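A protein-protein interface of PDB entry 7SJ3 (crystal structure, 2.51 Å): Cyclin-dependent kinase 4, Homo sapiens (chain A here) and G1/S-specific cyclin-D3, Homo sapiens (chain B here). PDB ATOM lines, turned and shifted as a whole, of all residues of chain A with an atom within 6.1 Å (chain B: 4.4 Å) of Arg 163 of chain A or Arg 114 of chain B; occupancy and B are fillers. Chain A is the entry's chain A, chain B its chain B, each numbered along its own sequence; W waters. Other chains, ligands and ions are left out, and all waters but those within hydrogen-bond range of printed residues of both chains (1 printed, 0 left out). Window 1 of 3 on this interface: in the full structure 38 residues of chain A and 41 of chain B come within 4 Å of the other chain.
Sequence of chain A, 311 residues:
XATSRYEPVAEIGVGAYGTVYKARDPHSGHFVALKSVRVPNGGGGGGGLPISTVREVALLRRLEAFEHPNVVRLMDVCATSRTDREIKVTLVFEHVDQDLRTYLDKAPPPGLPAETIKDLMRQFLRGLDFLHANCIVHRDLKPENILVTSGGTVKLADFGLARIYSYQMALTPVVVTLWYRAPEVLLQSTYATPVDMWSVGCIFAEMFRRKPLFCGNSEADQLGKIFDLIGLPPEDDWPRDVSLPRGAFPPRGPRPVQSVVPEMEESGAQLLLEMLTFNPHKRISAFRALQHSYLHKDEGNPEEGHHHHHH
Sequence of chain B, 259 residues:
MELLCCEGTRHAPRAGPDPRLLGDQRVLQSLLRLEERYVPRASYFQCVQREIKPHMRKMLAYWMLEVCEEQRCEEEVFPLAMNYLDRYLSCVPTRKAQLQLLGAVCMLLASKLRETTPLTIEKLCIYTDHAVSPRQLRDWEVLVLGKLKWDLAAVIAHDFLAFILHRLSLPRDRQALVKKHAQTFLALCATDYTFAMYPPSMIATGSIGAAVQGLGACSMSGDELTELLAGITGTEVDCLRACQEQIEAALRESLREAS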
ATOM      1  N   ARG A  55      -4.426 -18.091  15.734  1.00  0.00           N
ATOM      2  CA  ARG A  55      -4.498 -18.720  17.052  1.00  0.00           C
ATOM      3  C   ARG A  55      -4.860 -17.723  18.147  1.00  0.00           C
ATOM      4  O   ARG A  55      -5.744 -17.988  18.970  1.00  0.00           O
ATOM      5  CB  ARG A  55      -3.178 -19.403  17.383  1.00  0.00           C
ATOM      6  CG  ARG A  55      -2.970 -20.685  16.608  1.00  0.00           C
ATOM      7  CD  ARG A  55      -1.716 -21.364  17.059  1.00  0.00           C
ATOM      8  NE  ARG A  55      -1.411 -22.541  16.262  1.00  0.00           N
ATOM      9  CZ  ARG A  55      -0.266 -23.205  16.357  1.00  0.00           C
ATOM     10  NH1 ARG A  55       0.661 -22.789  17.214  1.00  0.00           N
ATOM     11  NH2 ARG A  55      -0.046 -24.273  15.599  1.00  0.00           N
ATOM     12  N   LEU A  59      -8.343 -17.998  20.376  1.00  0.00           N
ATOM     13  CA  LEU A  59      -8.344 -18.252  21.815  1.00  0.00           C
ATOM     14  C   LEU A  59      -9.058 -17.144  22.578  1.00  0.00           C
ATOM     15  O   LEU A  59      -9.801 -17.416  23.530  1.00  0.00           O
ATOM     16  CB  LEU A  59      -6.914 -18.397  22.328  1.00  0.00           C
ATOM     17  CG  LEU A  59      -6.182 -19.656  21.879  1.00  0.00           C
ATOM     18  CD1 LEU A  59      -4.860 -19.763  22.611  1.00  0.00           C
ATOM     19  CD2 LEU A  59      -7.043 -20.884  22.103  1.00  0.00           C
ATOM     20  N   ARG A  62     -12.761 -17.501  22.179  1.00  0.00           N
ATOM     21  CA  ARG A  62     -13.305 -18.547  23.040  1.00  0.00           C
ATOM     22  C   ARG A  62     -13.413 -18.054  24.478  1.00  0.00           C
ATOM     23  O   ARG A  62     -14.400 -18.339  25.166  1.00  0.00           O
ATOM     24  CB  ARG A  62     -12.429 -19.804  22.975  1.00  0.00           C
ATOM     25  CG  ARG A  62     -12.872 -20.913  23.935  1.00  0.00           C
ATOM     26  CD  ARG A  62     -11.771 -21.942  24.189  1.00  0.00           C
ATOM     27  NE  ARG A  62     -11.772 -23.045  23.234  1.00  0.00           N
ATOM     28  CZ  ARG A  62     -11.971 -24.320  23.555  1.00  0.00           C
ATOM     29  NH1 ARG A  62     -12.171 -24.671  24.817  1.00  0.00           N
ATOM     30  NH2 ARG A  62     -11.951 -25.251  22.614  1.00  0.00           N
ATOM     31  N   CYS A 135      -8.270 -25.187  29.433  1.00  0.00           N
ATOM     32  CA  CYS A 135      -7.382 -25.965  28.567  1.00  0.00           C
ATOM     33  C   CYS A 135      -6.382 -25.111  27.806  1.00  0.00           C
ATOM     34  O   CYS A 135      -5.893 -25.525  26.748  1.00  0.00           O
ATOM     35  CB  CYS A 135      -8.166 -26.812  27.557  1.00  0.00           C
ATOM     36  SG  CYS A 135      -8.556 -28.459  28.092  1.00  0.00           S
ATOM     37  N   ILE A 136      -6.054 -23.929  28.308  1.00  0.00           N
ATOM     38  CA  ILE A 136      -5.195 -22.993  27.597  1.00  0.00           C
ATOM     39  C   ILE A 136      -3.875 -22.887  28.341  1.00  0.00           C
ATOM     40  O   ILE A 136      -3.852 -22.698  29.563  1.00  0.00           O
ATOM     41  CB  ILE A 136      -5.858 -21.616  27.439  1.00  0.00           C
ATOM     42  CG1 ILE A 136      -6.990 -21.711  26.412  1.00  0.00           C
ATOM     43  CG2 ILE A 136      -4.827 -20.576  27.039  1.00  0.00           C
ATOM     44  CD1 ILE A 136      -7.866 -20.497  26.345  1.00  0.00           C
ATOM     45  N   VAL A 137      -2.780 -23.026  27.602  1.00  0.00           N
ATOM     46  CA  VAL A 137      -1.438 -22.787  28.107  1.00  0.00           C
ATOM     47  C   VAL A 137      -0.936 -21.510  27.456  1.00  0.00           C
ATOM     48  O   VAL A 137      -1.072 -21.333  26.239  1.00  0.00           O
ATOM     49  CB  VAL A 137      -0.502 -23.970  27.809  1.00  0.00           C
ATOM     50  CG1 VAL A 137       0.820 -23.790  28.531  1.00  0.00           C
ATOM     51  CG2 VAL A 137      -1.168 -25.283  28.207  1.00  0.00           C
ATOM     52  N   HIS A 138      -0.370 -20.613  28.266  1.00  0.00           N
ATOM     53  CA  HIS A 138       0.046 -19.308  27.763  1.00  0.00           C
ATOM     54  C   HIS A 138       1.366 -19.393  27.000  1.00  0.00           C
ATOM     55  O   HIS A 138       1.464 -18.920  25.860  1.00  0.00           O
ATOM     56  CB  HIS A 138       0.155 -18.315  28.921  1.00  0.00           C
ATOM     57  CG  HIS A 138       0.330 -16.895  28.482  1.00  0.00           C
ATOM     58  ND1 HIS A 138       1.552 -16.382  28.109  1.00  0.00           N
ATOM     59  CD2 HIS A 138      -0.558 -15.879  28.359  1.00  0.00           C
ATOM     60  CE1 HIS A 138       1.411 -15.113  27.772  1.00  0.00           C
ATOM     61  NE2 HIS A 138       0.140 -14.781  27.916  1.00  0.00           N
ATOM     62  N   ARG A 139       2.400 -19.952  27.637  1.00  0.00           N
ATOM     63  CA  ARG A 139       3.707 -20.226  27.044  1.00  0.00           C
ATOM     64  C   ARG A 139       4.502 -18.961  26.749  1.00  0.00           C
ATOM     65  O   ARG A 139       5.484 -19.013  25.999  1.00  0.00           O
ATOM     66  CB  ARG A 139       3.604 -21.075  25.770  1.00  0.00           C
ATOM     67  CG  ARG A 139       2.854 -22.381  25.942  1.00  0.00           C
ATOM     68  CD  ARG A 139       3.022 -23.267  24.719  1.00  0.00           C
ATOM     69  NE  ARG A 139       2.589 -22.602  23.491  1.00  0.00           N
ATOM     70  CZ  ARG A 139       2.668 -23.139  22.277  1.00  0.00           C
ATOM     71  NH1 ARG A 139       3.169 -24.361  22.120  1.00  0.00           N
ATOM     72  NH2 ARG A 139       2.245 -22.458  21.218  1.00  0.00           N
ATOM     73  N   PHE A 159      -1.595 -13.391  23.710  1.00  0.00           N
ATOM     74  CA  PHE A 159      -1.920 -14.798  23.526  1.00  0.00           C
ATOM     75  C   PHE A 159      -1.487 -15.320  22.162  1.00  0.00           C
ATOM     76  O   PHE A 159      -1.977 -16.360  21.711  1.00  0.00           O
ATOM     77  CB  PHE A 159      -3.417 -15.016  23.751  1.00  0.00           C
ATOM     78  CG  PHE A 159      -3.835 -14.842  25.179  1.00  0.00           C
ATOM     79  CD1 PHE A 159      -3.995 -13.579  25.731  1.00  0.00           C
ATOM     80  CD2 PHE A 159      -4.062 -15.951  25.979  1.00  0.00           C
ATOM     81  CE1 PHE A 159      -4.364 -13.424  27.058  1.00  0.00           C
ATOM     82  CE2 PHE A 159      -4.440 -15.807  27.302  1.00  0.00           C
ATOM     83  CZ  PHE A 159      -4.592 -14.539  27.844  1.00  0.00           C
ATOM     84  N   LEU A 161       1.332 -16.719  21.416  1.00  0.00           N
ATOM     85  CA  LEU A 161       2.071 -17.967  21.579  1.00  0.00           C
ATOM     86  C   LEU A 161       1.278 -19.066  22.279  1.00  0.00           C
ATOM     87  O   LEU A 161       1.819 -20.154  22.507  1.00  0.00           O
ATOM     88  CB  LEU A 161       3.368 -17.706  22.352  1.00  0.00           C
ATOM     89  CG  LEU A 161       4.652 -18.025  21.589  1.00  0.00           C
ATOM     90  CD1 LEU A 161       5.436 -16.739  21.366  1.00  0.00           C
ATOM     91  CD2 LEU A 161       5.491 -19.074  22.318  1.00  0.00           C
ATOM     92  N   ALA A 162       0.031 -18.807  22.642  1.00  0.00           N
ATOM     93  CA  ALA A 162      -0.782 -19.701  23.450  1.00  0.00           C
ATOM     94  C   ALA A 162      -1.481 -20.747  22.585  1.00  0.00           C
ATOM     95  O   ALA A 162      -1.651 -20.581  21.375  1.00  0.00           O
ATOM     96  CB  ALA A 162      -1.812 -18.905  24.255  1.00  0.00           C
ATOM     97  N   ARG A 163      -1.870 -21.848  23.227  1.00  0.00           N
ATOM     98  CA  ARG A 163      -2.524 -22.949  22.534  1.00  0.00           C
ATOM     99  C   ARG A 163      -3.470 -23.659  23.484  1.00  0.00           C
ATOM    100  O   ARG A 163      -3.276 -23.656  24.702  1.00  0.00           O
ATOM    101  CB  ARG A 163      -1.517 -23.988  22.002  1.00  0.00           C
ATOM    102  CG  ARG A 163      -0.767 -23.609  20.744  1.00  0.00           C
ATOM    103  CD  ARG A 163       0.045 -24.789  20.222  1.00  0.00           C
ATOM    104  NE  ARG A 163      -0.761 -25.796  19.533  1.00  0.00           N
ATOM    105  CZ  ARG A 163      -0.255 -26.887  18.961  1.00  0.00           C
ATOM    106  NH1 ARG A 163       1.050 -27.114  19.002  1.00  0.00           N
ATOM    107  NH2 ARG A 163      -1.047 -27.755  18.355  1.00  0.00           N
ATOM    108  N   ILE A 164      -4.500 -24.268  22.900  1.00  0.00           N
ATOM    109  CA  ILE A 164      -5.255 -25.299  23.592  1.00  0.00           C
ATOM    110  C   ILE A 164      -4.417 -26.570  23.632  1.00  0.00           C
ATOM    111  O   ILE A 164      -3.918 -27.036  22.599  1.00  0.00           O
ATOM    112  CB  ILE A 164      -6.602 -25.533  22.894  1.00  0.00           C
ATOM    113  CG1 ILE A 164      -7.528 -24.335  23.101  1.00  0.00           C
ATOM    114  CG2 ILE A 164      -7.257 -26.806  23.403  1.00  0.00           C
ATOM    115  CD1 ILE A 164      -8.809 -24.427  22.303  1.00  0.00           C
ATOM    116  N   TYR A 165      -4.246 -27.124  24.826  1.00  0.00           N
ATOM    117  CA  TYR A 165      -3.441 -28.318  25.019  1.00  0.00           C
ATOM    118  C   TYR A 165      -4.314 -29.556  24.838  1.00  0.00           C
ATOM    119  O   TYR A 165      -5.292 -29.744  25.570  1.00  0.00           O
ATOM    120  CB  TYR A 165      -2.777 -28.309  26.394  1.00  0.00           C
ATOM    121  CG  TYR A 165      -1.720 -29.379  26.550  1.00  0.00           C
ATOM    122  CD1 TYR A 165      -0.405 -29.138  26.179  1.00  0.00           C
ATOM    123  CD2 TYR A 165      -2.042 -30.630  27.056  1.00  0.00           C
ATOM    124  CE1 TYR A 165       0.569 -30.114  26.315  1.00  0.00           C
ATOM    125  CE2 TYR A 165      -1.077 -31.614  27.195  1.00  0.00           C
ATOM    126  CZ  TYR A 165       0.229 -31.351  26.823  1.00  0.00           C
ATOM    127  OH  TYR A 165       1.192 -32.328  26.960  1.00  0.00           O
ATOM    128  N   SER A 166      -3.976 -30.380  23.846  1.00  0.00           N
ATOM    129  CA  SER A 166      -4.744 -31.573  23.503  1.00  0.00           C
ATOM    130  C   SER A 166      -3.810 -32.774  23.500  1.00  0.00           C
ATOM    131  O   SER A 166      -2.827 -32.795  22.754  1.00  0.00           O
ATOM    132  CB  SER A 166      -5.438 -31.427  22.146  1.00  0.00           C
ATOM    133  OG  SER A 166      -6.265 -30.278  22.115  1.00  0.00           O
ATOM    134  N   MET A 169      -1.229 -34.219  20.618  1.00  0.00           N
ATOM    135  CA  MET A 169      -0.891 -33.266  19.567  1.00  0.00           C
ATOM    136  C   MET A 169       0.609 -32.978  19.550  1.00  0.00           C
ATOM    137  O   MET A 169       1.301 -33.089  20.566  1.00  0.00           O
ATOM    138  CB  MET A 169      -1.656 -31.957  19.742  1.00  0.00           C
ATOM    139  CG  MET A 169      -1.088 -31.036  20.804  1.00  0.00           C
ATOM    140  SD  MET A 169      -2.063 -29.536  20.995  1.00  0.00           S
ATOM    141  CE  MET A 169      -1.051 -28.609  22.147  1.00  0.00           C
ATOM    142  N   ALA A 170       1.108 -32.600  18.375  1.00  0.00           N
ATOM    143  CA  ALA A 170       2.495 -32.173  18.256  1.00  0.00           C
ATOM    144  C   ALA A 170       2.684 -30.814  18.924  1.00  0.00           C
ATOM    145  O   ALA A 170       1.795 -29.958  18.905  1.00  0.00           O
ATOM    146  CB  ALA A 170       2.913 -32.108  16.788  1.00  0.00           C
ATOM    147  N   LEU A 171       3.862 -30.618  19.515  1.00  0.00           N
ATOM    148  CA  LEU A 171       4.162 -29.374  20.224  1.00  0.00           C
ATOM    149  C   LEU A 171       5.315 -28.611  19.586  1.00  0.00           C
ATOM    150  O   LEU A 171       6.285 -29.207  19.113  1.00  0.00           O
ATOM    151  CB  LEU A 171       4.501 -29.658  21.693  1.00  0.00           C
ATOM    152  CG  LEU A 171       3.369 -30.046  22.646  1.00  0.00           C
ATOM    153  CD1 LEU A 171       3.928 -30.615  23.947  1.00  0.00           C
ATOM    154  CD2 LEU A 171       2.474 -28.851  22.915  1.00  0.00           C
ATOM    155  N   TPO A 172       5.200 -27.285  19.578  1.00  0.00           N
ATOM    156  CA  TPO A 172       6.306 -26.421  19.183  1.00  0.00           C
ATOM    157  CB  TPO A 172       5.830 -24.968  19.027  1.00  0.00           C
ATOM    158  CG2 TPO A 172       7.035 -24.049  18.833  1.00  0.00           C
ATOM    159  OG1 TPO A 172       5.012 -24.888  17.855  1.00  0.00           O
ATOM    160  P   TPO A 172       3.455 -24.688  18.236  1.00  0.00           P
ATOM    161  O1P TPO A 172       3.076 -25.562  19.536  1.00  0.00           O
ATOM    162  O2P TPO A 172       2.560 -25.174  16.989  1.00  0.00           O
ATOM    163  O3P TPO A 172       3.157 -23.268  18.537  1.00  0.00           O
ATOM    164  C   TPO A 172       7.426 -26.541  20.224  1.00  0.00           C
ATOM    165  O   TPO A 172       7.238 -26.200  21.391  1.00  0.00           O
ATOM    166  N   GLU B  76      -8.367 -33.999  14.683  1.00  0.00           N
ATOM    167  CA  GLU B  76      -9.349 -32.936  14.887  1.00  0.00           C
ATOM    168  C   GLU B  76      -9.580 -32.071  13.657  1.00  0.00           C
ATOM    169  O   GLU B  76     -10.578 -31.346  13.621  1.00  0.00           O
ATOM    170  CB  GLU B  76      -8.985 -32.050  16.090  1.00  0.00           C
ATOM    171  CG  GLU B  76      -8.154 -32.716  17.196  1.00  0.00           C
ATOM    172  CD  GLU B  76      -6.683 -32.787  16.883  1.00  0.00           C
ATOM    173  OE1 GLU B  76      -6.088 -31.727  16.612  1.00  0.00           O
ATOM    174  OE2 GLU B  76      -6.113 -33.891  16.953  1.00  0.00           O
ATOM    175  N   LEU B  80     -13.274 -30.334  12.680  1.00  0.00           N
ATOM    176  CA  LEU B  80     -13.247 -28.895  12.910  1.00  0.00           C
ATOM    177  C   LEU B  80     -13.549 -28.133  11.621  1.00  0.00           C
ATOM    178  O   LEU B  80     -14.251 -27.116  11.642  1.00  0.00           O
ATOM    179  CB  LEU B  80     -11.896 -28.510  13.507  1.00  0.00           C
ATOM    180  CG  LEU B  80     -11.776 -27.112  14.084  1.00  0.00           C
ATOM    181  CD1 LEU B  80     -12.887 -26.886  15.103  1.00  0.00           C
ATOM    182  CD2 LEU B  80     -10.425 -26.995  14.753  1.00  0.00           C
ATOM    183  N   ALA B 110      -8.801 -24.715   9.975  1.00  0.00           N
ATOM    184  CA  ALA B 110      -8.751 -25.728  11.028  1.00  0.00           C
ATOM    185  C   ALA B 110      -7.323 -26.215  11.229  1.00  0.00           C
ATOM    186  O   ALA B 110      -6.864 -26.386  12.366  1.00  0.00           O
ATOM    187  CB  ALA B 110      -9.686 -26.891  10.700  1.00  0.00           C
ATOM    188  N   SER B 111      -6.611 -26.455  10.126  1.00  0.00           N
ATOM    189  CA  SER B 111      -5.232 -26.928  10.196  1.00  0.00           C
ATOM    190  C   SER B 111      -4.316 -25.866  10.798  1.00  0.00           C
ATOM    191  O   SER B 111      -3.440 -26.182  11.614  1.00  0.00           O
ATOM    192  CB  SER B 111      -4.750 -27.322   8.800  1.00  0.00           C
ATOM    193  OG  SER B 111      -3.396 -27.732   8.830  1.00  0.00           O
ATOM    194  N   LYS B 112      -4.457 -24.609  10.362  1.00  0.00           N
ATOM    195  CA  LYS B 112      -3.636 -23.544  10.929  1.00  0.00           C
ATOM    196  C   LYS B 112      -3.845 -23.420  12.432  1.00  0.00           C
ATOM    197  O   LYS B 112      -2.901 -23.130  13.180  1.00  0.00           O
ATOM    198  CB  LYS B 112      -3.953 -22.205  10.257  1.00  0.00           C
ATOM    199  CG  LYS B 112      -3.358 -22.016   8.886  1.00  0.00           C
ATOM    200  CD  LYS B 112      -3.659 -20.611   8.337  1.00  0.00           C
ATOM    201  CE  LYS B 112      -2.897 -20.375   7.046  1.00  0.00           C
ATOM    202  NZ  LYS B 112      -3.038 -19.003   6.497  1.00  0.00           N
ATOM    203  N   LEU B 113      -5.080 -23.635  12.896  1.00  0.00           N
ATOM    204  CA  LEU B 113      -5.358 -23.516  14.325  1.00  0.00           C
ATOM    205  C   LEU B 113      -4.756 -24.666  15.130  1.00  0.00           C
ATOM    206  O   LEU B 113      -4.163 -24.431  16.190  1.00  0.00           O
ATOM    207  CB  LEU B 113      -6.867 -23.382  14.565  1.00  0.00           C
ATOM    208  CG  LEU B 113      -7.282 -23.279  16.038  1.00  0.00           C
ATOM    209  CD1 LEU B 113      -6.739 -21.994  16.625  1.00  0.00           C
ATOM    210  CD2 LEU B 113      -8.793 -23.291  16.194  1.00  0.00           C
ATOM    211  N   ARG B 114      -4.866 -25.909  14.640  1.00  0.00           N
ATOM    212  CA  ARG B 114      -4.600 -27.078  15.472  1.00  0.00           C
ATOM    213  C   ARG B 114      -3.288 -27.804  15.194  1.00  0.00           C
ATOM    214  O   ARG B 114      -2.903 -28.653  16.002  1.00  0.00           O
ATOM    215  CB  ARG B 114      -5.737 -28.109  15.361  1.00  0.00           C
ATOM    216  CG  ARG B 114      -7.068 -27.669  15.923  1.00  0.00           C
ATOM    217  CD  ARG B 114      -7.043 -27.615  17.446  1.00  0.00           C
ATOM    218  NE  ARG B 114      -8.385 -27.436  17.992  1.00  0.00           N
ATOM    219  CZ  ARG B 114      -9.077 -28.390  18.610  1.00  0.00           C
ATOM    220  NH1 ARG B 114      -8.545 -29.598  18.785  1.00  0.00           N
ATOM    221  NH2 ARG B 114     -10.299 -28.129  19.057  1.00  0.00           N
ATOM    222  N   GLU B 115      -2.596 -27.523  14.094  1.00  0.00           N
ATOM    223  CA  GLU B 115      -1.454 -28.327  13.669  1.00  0.00           C
ATOM    224  C   GLU B 115      -0.159 -27.527  13.718  1.00  0.00           C
ATOM    225  O   GLU B 115      -0.111 -26.374  13.278  1.00  0.00           O
ATOM    226  CB  GLU B 115      -1.639 -28.874  12.253  1.00  0.00           C
ATOM    227  CG  GLU B 115      -2.801 -29.820  12.097  1.00  0.00           C
ATOM    228  CD  GLU B 115      -2.664 -30.721  10.885  1.00  0.00           C
ATOM    229  OE1 GLU B 115      -2.865 -30.235   9.751  1.00  0.00           O
ATOM    230  OE2 GLU B 115      -2.356 -31.920  11.065  1.00  0.00           O
ATOM    231  N   THR B 116       0.892 -28.150  14.258  1.00  0.00           N
ATOM    232  CA  THR B 116       2.194 -27.501  14.254  1.00  0.00           C
ATOM    233  C   THR B 116       2.755 -27.401  12.842  1.00  0.00           C
ATOM    234  O   THR B 116       3.398 -26.403  12.504  1.00  0.00           O
ATOM    235  CB  THR B 116       3.174 -28.268  15.144  1.00  0.00           C
ATOM    236  OG1 THR B 116       2.746 -28.200  16.507  1.00  0.00           O
ATOM    237  N   ALA B 154     -13.381 -23.889  18.208  1.00  0.00           N
ATOM    238  CA  ALA B 154     -14.593 -24.610  18.552  1.00  0.00           C
ATOM    239  C   ALA B 154     -14.273 -25.859  19.368  1.00  0.00           C
ATOM    240  O   ALA B 154     -13.183 -26.432  19.275  1.00  0.00           O
ATOM    241  CB  ALA B 154     -15.359 -24.994  17.284  1.00  0.00           C
ATOM    242  N   ILE B 156     -15.135 -29.617  19.559  1.00  0.00           N
ATOM    243  CA  ILE B 156     -15.648 -30.694  18.729  1.00  0.00           C
ATOM    244  C   ILE B 156     -15.520 -31.994  19.513  1.00  0.00           C
ATOM    245  O   ILE B 156     -14.907 -32.044  20.579  1.00  0.00           O
ATOM    246  CB  ILE B 156     -14.926 -30.779  17.366  1.00  0.00           C
ATOM    247  CG1 ILE B 156     -13.413 -30.637  17.548  1.00  0.00           C
ATOM    248  CG2 ILE B 156     -15.465 -29.734  16.395  1.00  0.00           C
ATOM    249  CD1 ILE B 156     -12.643 -31.836  17.173  1.00  0.00           C
ATOM    250  N   ASP B 159     -12.330 -33.464  21.161  1.00  0.00           N
ATOM    251  CA  ASP B 159     -11.812 -32.829  22.369  1.00  0.00           C
ATOM    252  C   ASP B 159     -12.251 -33.537  23.652  1.00  0.00           C
ATOM    253  O   ASP B 159     -11.572 -33.414  24.677  1.00  0.00           O
ATOM    254  CB  ASP B 159     -12.222 -31.352  22.403  1.00  0.00           C
ATOM    255  CG  ASP B 159     -11.646 -30.565  21.245  1.00  0.00           C
ATOM    256  OD1 ASP B 159     -10.506 -30.869  20.828  1.00  0.00           O
ATOM    257  OD2 ASP B 159     -12.335 -29.648  20.744  1.00  0.00           O
HETATM  258  O   HOH W   1      -0.350 -30.175  17.027  1.00  0.00           O
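The guanidinium group (NH1) of Arg 55 of chain A sits close to O3P of TPO 172 of chain A, at 2.9 Å. The backbone carbonyl oxygen (O) of Arg 163 of chain A is in hydrogen-bond range of the backbone NH (N) of Val 137 of chain A (3.0 Å). NH1 of Arg 163 of chain A is in hydrogen-bond range of O of Ala 170 of chain A, 2.9 Å away. The guanidinium group (NH1) of Arg 163 of chain A sits close to O1P of TPO 172 of chain A (2.6 Å). The side-chain carboxylate of Glu 76 of chain B is in salt-bridge range of the guanidinium group of Arg 114 of chain B (3.9 Å). The side-chain carboxylate of Glu 115 of chain B sits at hydrogen-bond distance from the side-chain hydroxyl of Ser 111 of chain B, 2.7 Å away.
Water W1 lies within hydrogen-bond range of the guanidinium group (NH2) of Arg 163 of chain A (2.8 Å), the backbone carbonyl oxygen (O) of Ala 170 of chain A (2.9 Å) and the backbone carbonyl oxygen (O) of Arg 114 of chain B (3.1 Å).
Printed residues of chain B that touch a printed residue of chain A: Lys 112, Leu 113, Arg 114, Glu 115, Thr 116 and Ala 154. Among the printed residues, no Asp or Glu carboxylate lies within 4 Å of a Lys or Arg side-chain nitrogen of the other chain.
O of Lys 112 of chain B lies within hydrogen-bond range of NE of Arg 55 of chain A (3.5 Å). The backbone carbonyl oxygen (O) of Leu 113 of chain B lies within hydrogen-bond range of the guanidinium group (NE) of Arg 55 of chain A (3.3 Å). The backbone carbonyl oxygen (O) of Glu 115 of chain B sits at hydrogen-bond distance from the guanidinium group (NH2) of Arg 55 of chain A (3.1 Å). The guanidinium group (NH2) of Arg 163 of chain A is in hydrogen-bond range of the backbone carbonyl oxygen (O) of Arg 114 of chain B, at 3.1 Å. NH1 of Arg 163 of chain A lies within hydrogen-bond range of OG1 of Thr 116 of chain B (3.2 Å). O of Ala 170 of chain A is in hydrogen-bond range of OG1 of Thr 116 of chain B, at 3.1 Å. The side-chain hydroxyl (OG1) of Thr 116 of chain B lies within hydrogen-bond range of O2P of TPO 172 of chain A, at 3.1 Å.
Of the printed residues of chain B, Arg 55 of chain A touches Lys 112, Leu 113 and Glu 115. Ile 136 of chain A touches none of the printed residues of chain B. Of chain B, only Arg 114 and Thr 116 come within 4 Å of Arg 163 of chain A. Ser 111 of chain B touches none of the printed residues of chain A. Of the printed residues of chain A, Ala 154 of chain B touches Arg 62. The nearest printed residue of chain B that does not touch Arg 163 of chain A is Glu 115 of chain B (4.5 Å). The nearest residue of chain A that does not touch Arg 114 of chain B is Ser 166 of chain A (4.1 Å).
Among the printed residues, merely in contact across the chains: Arg 62 of chain A with Ala 154 of chain B.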
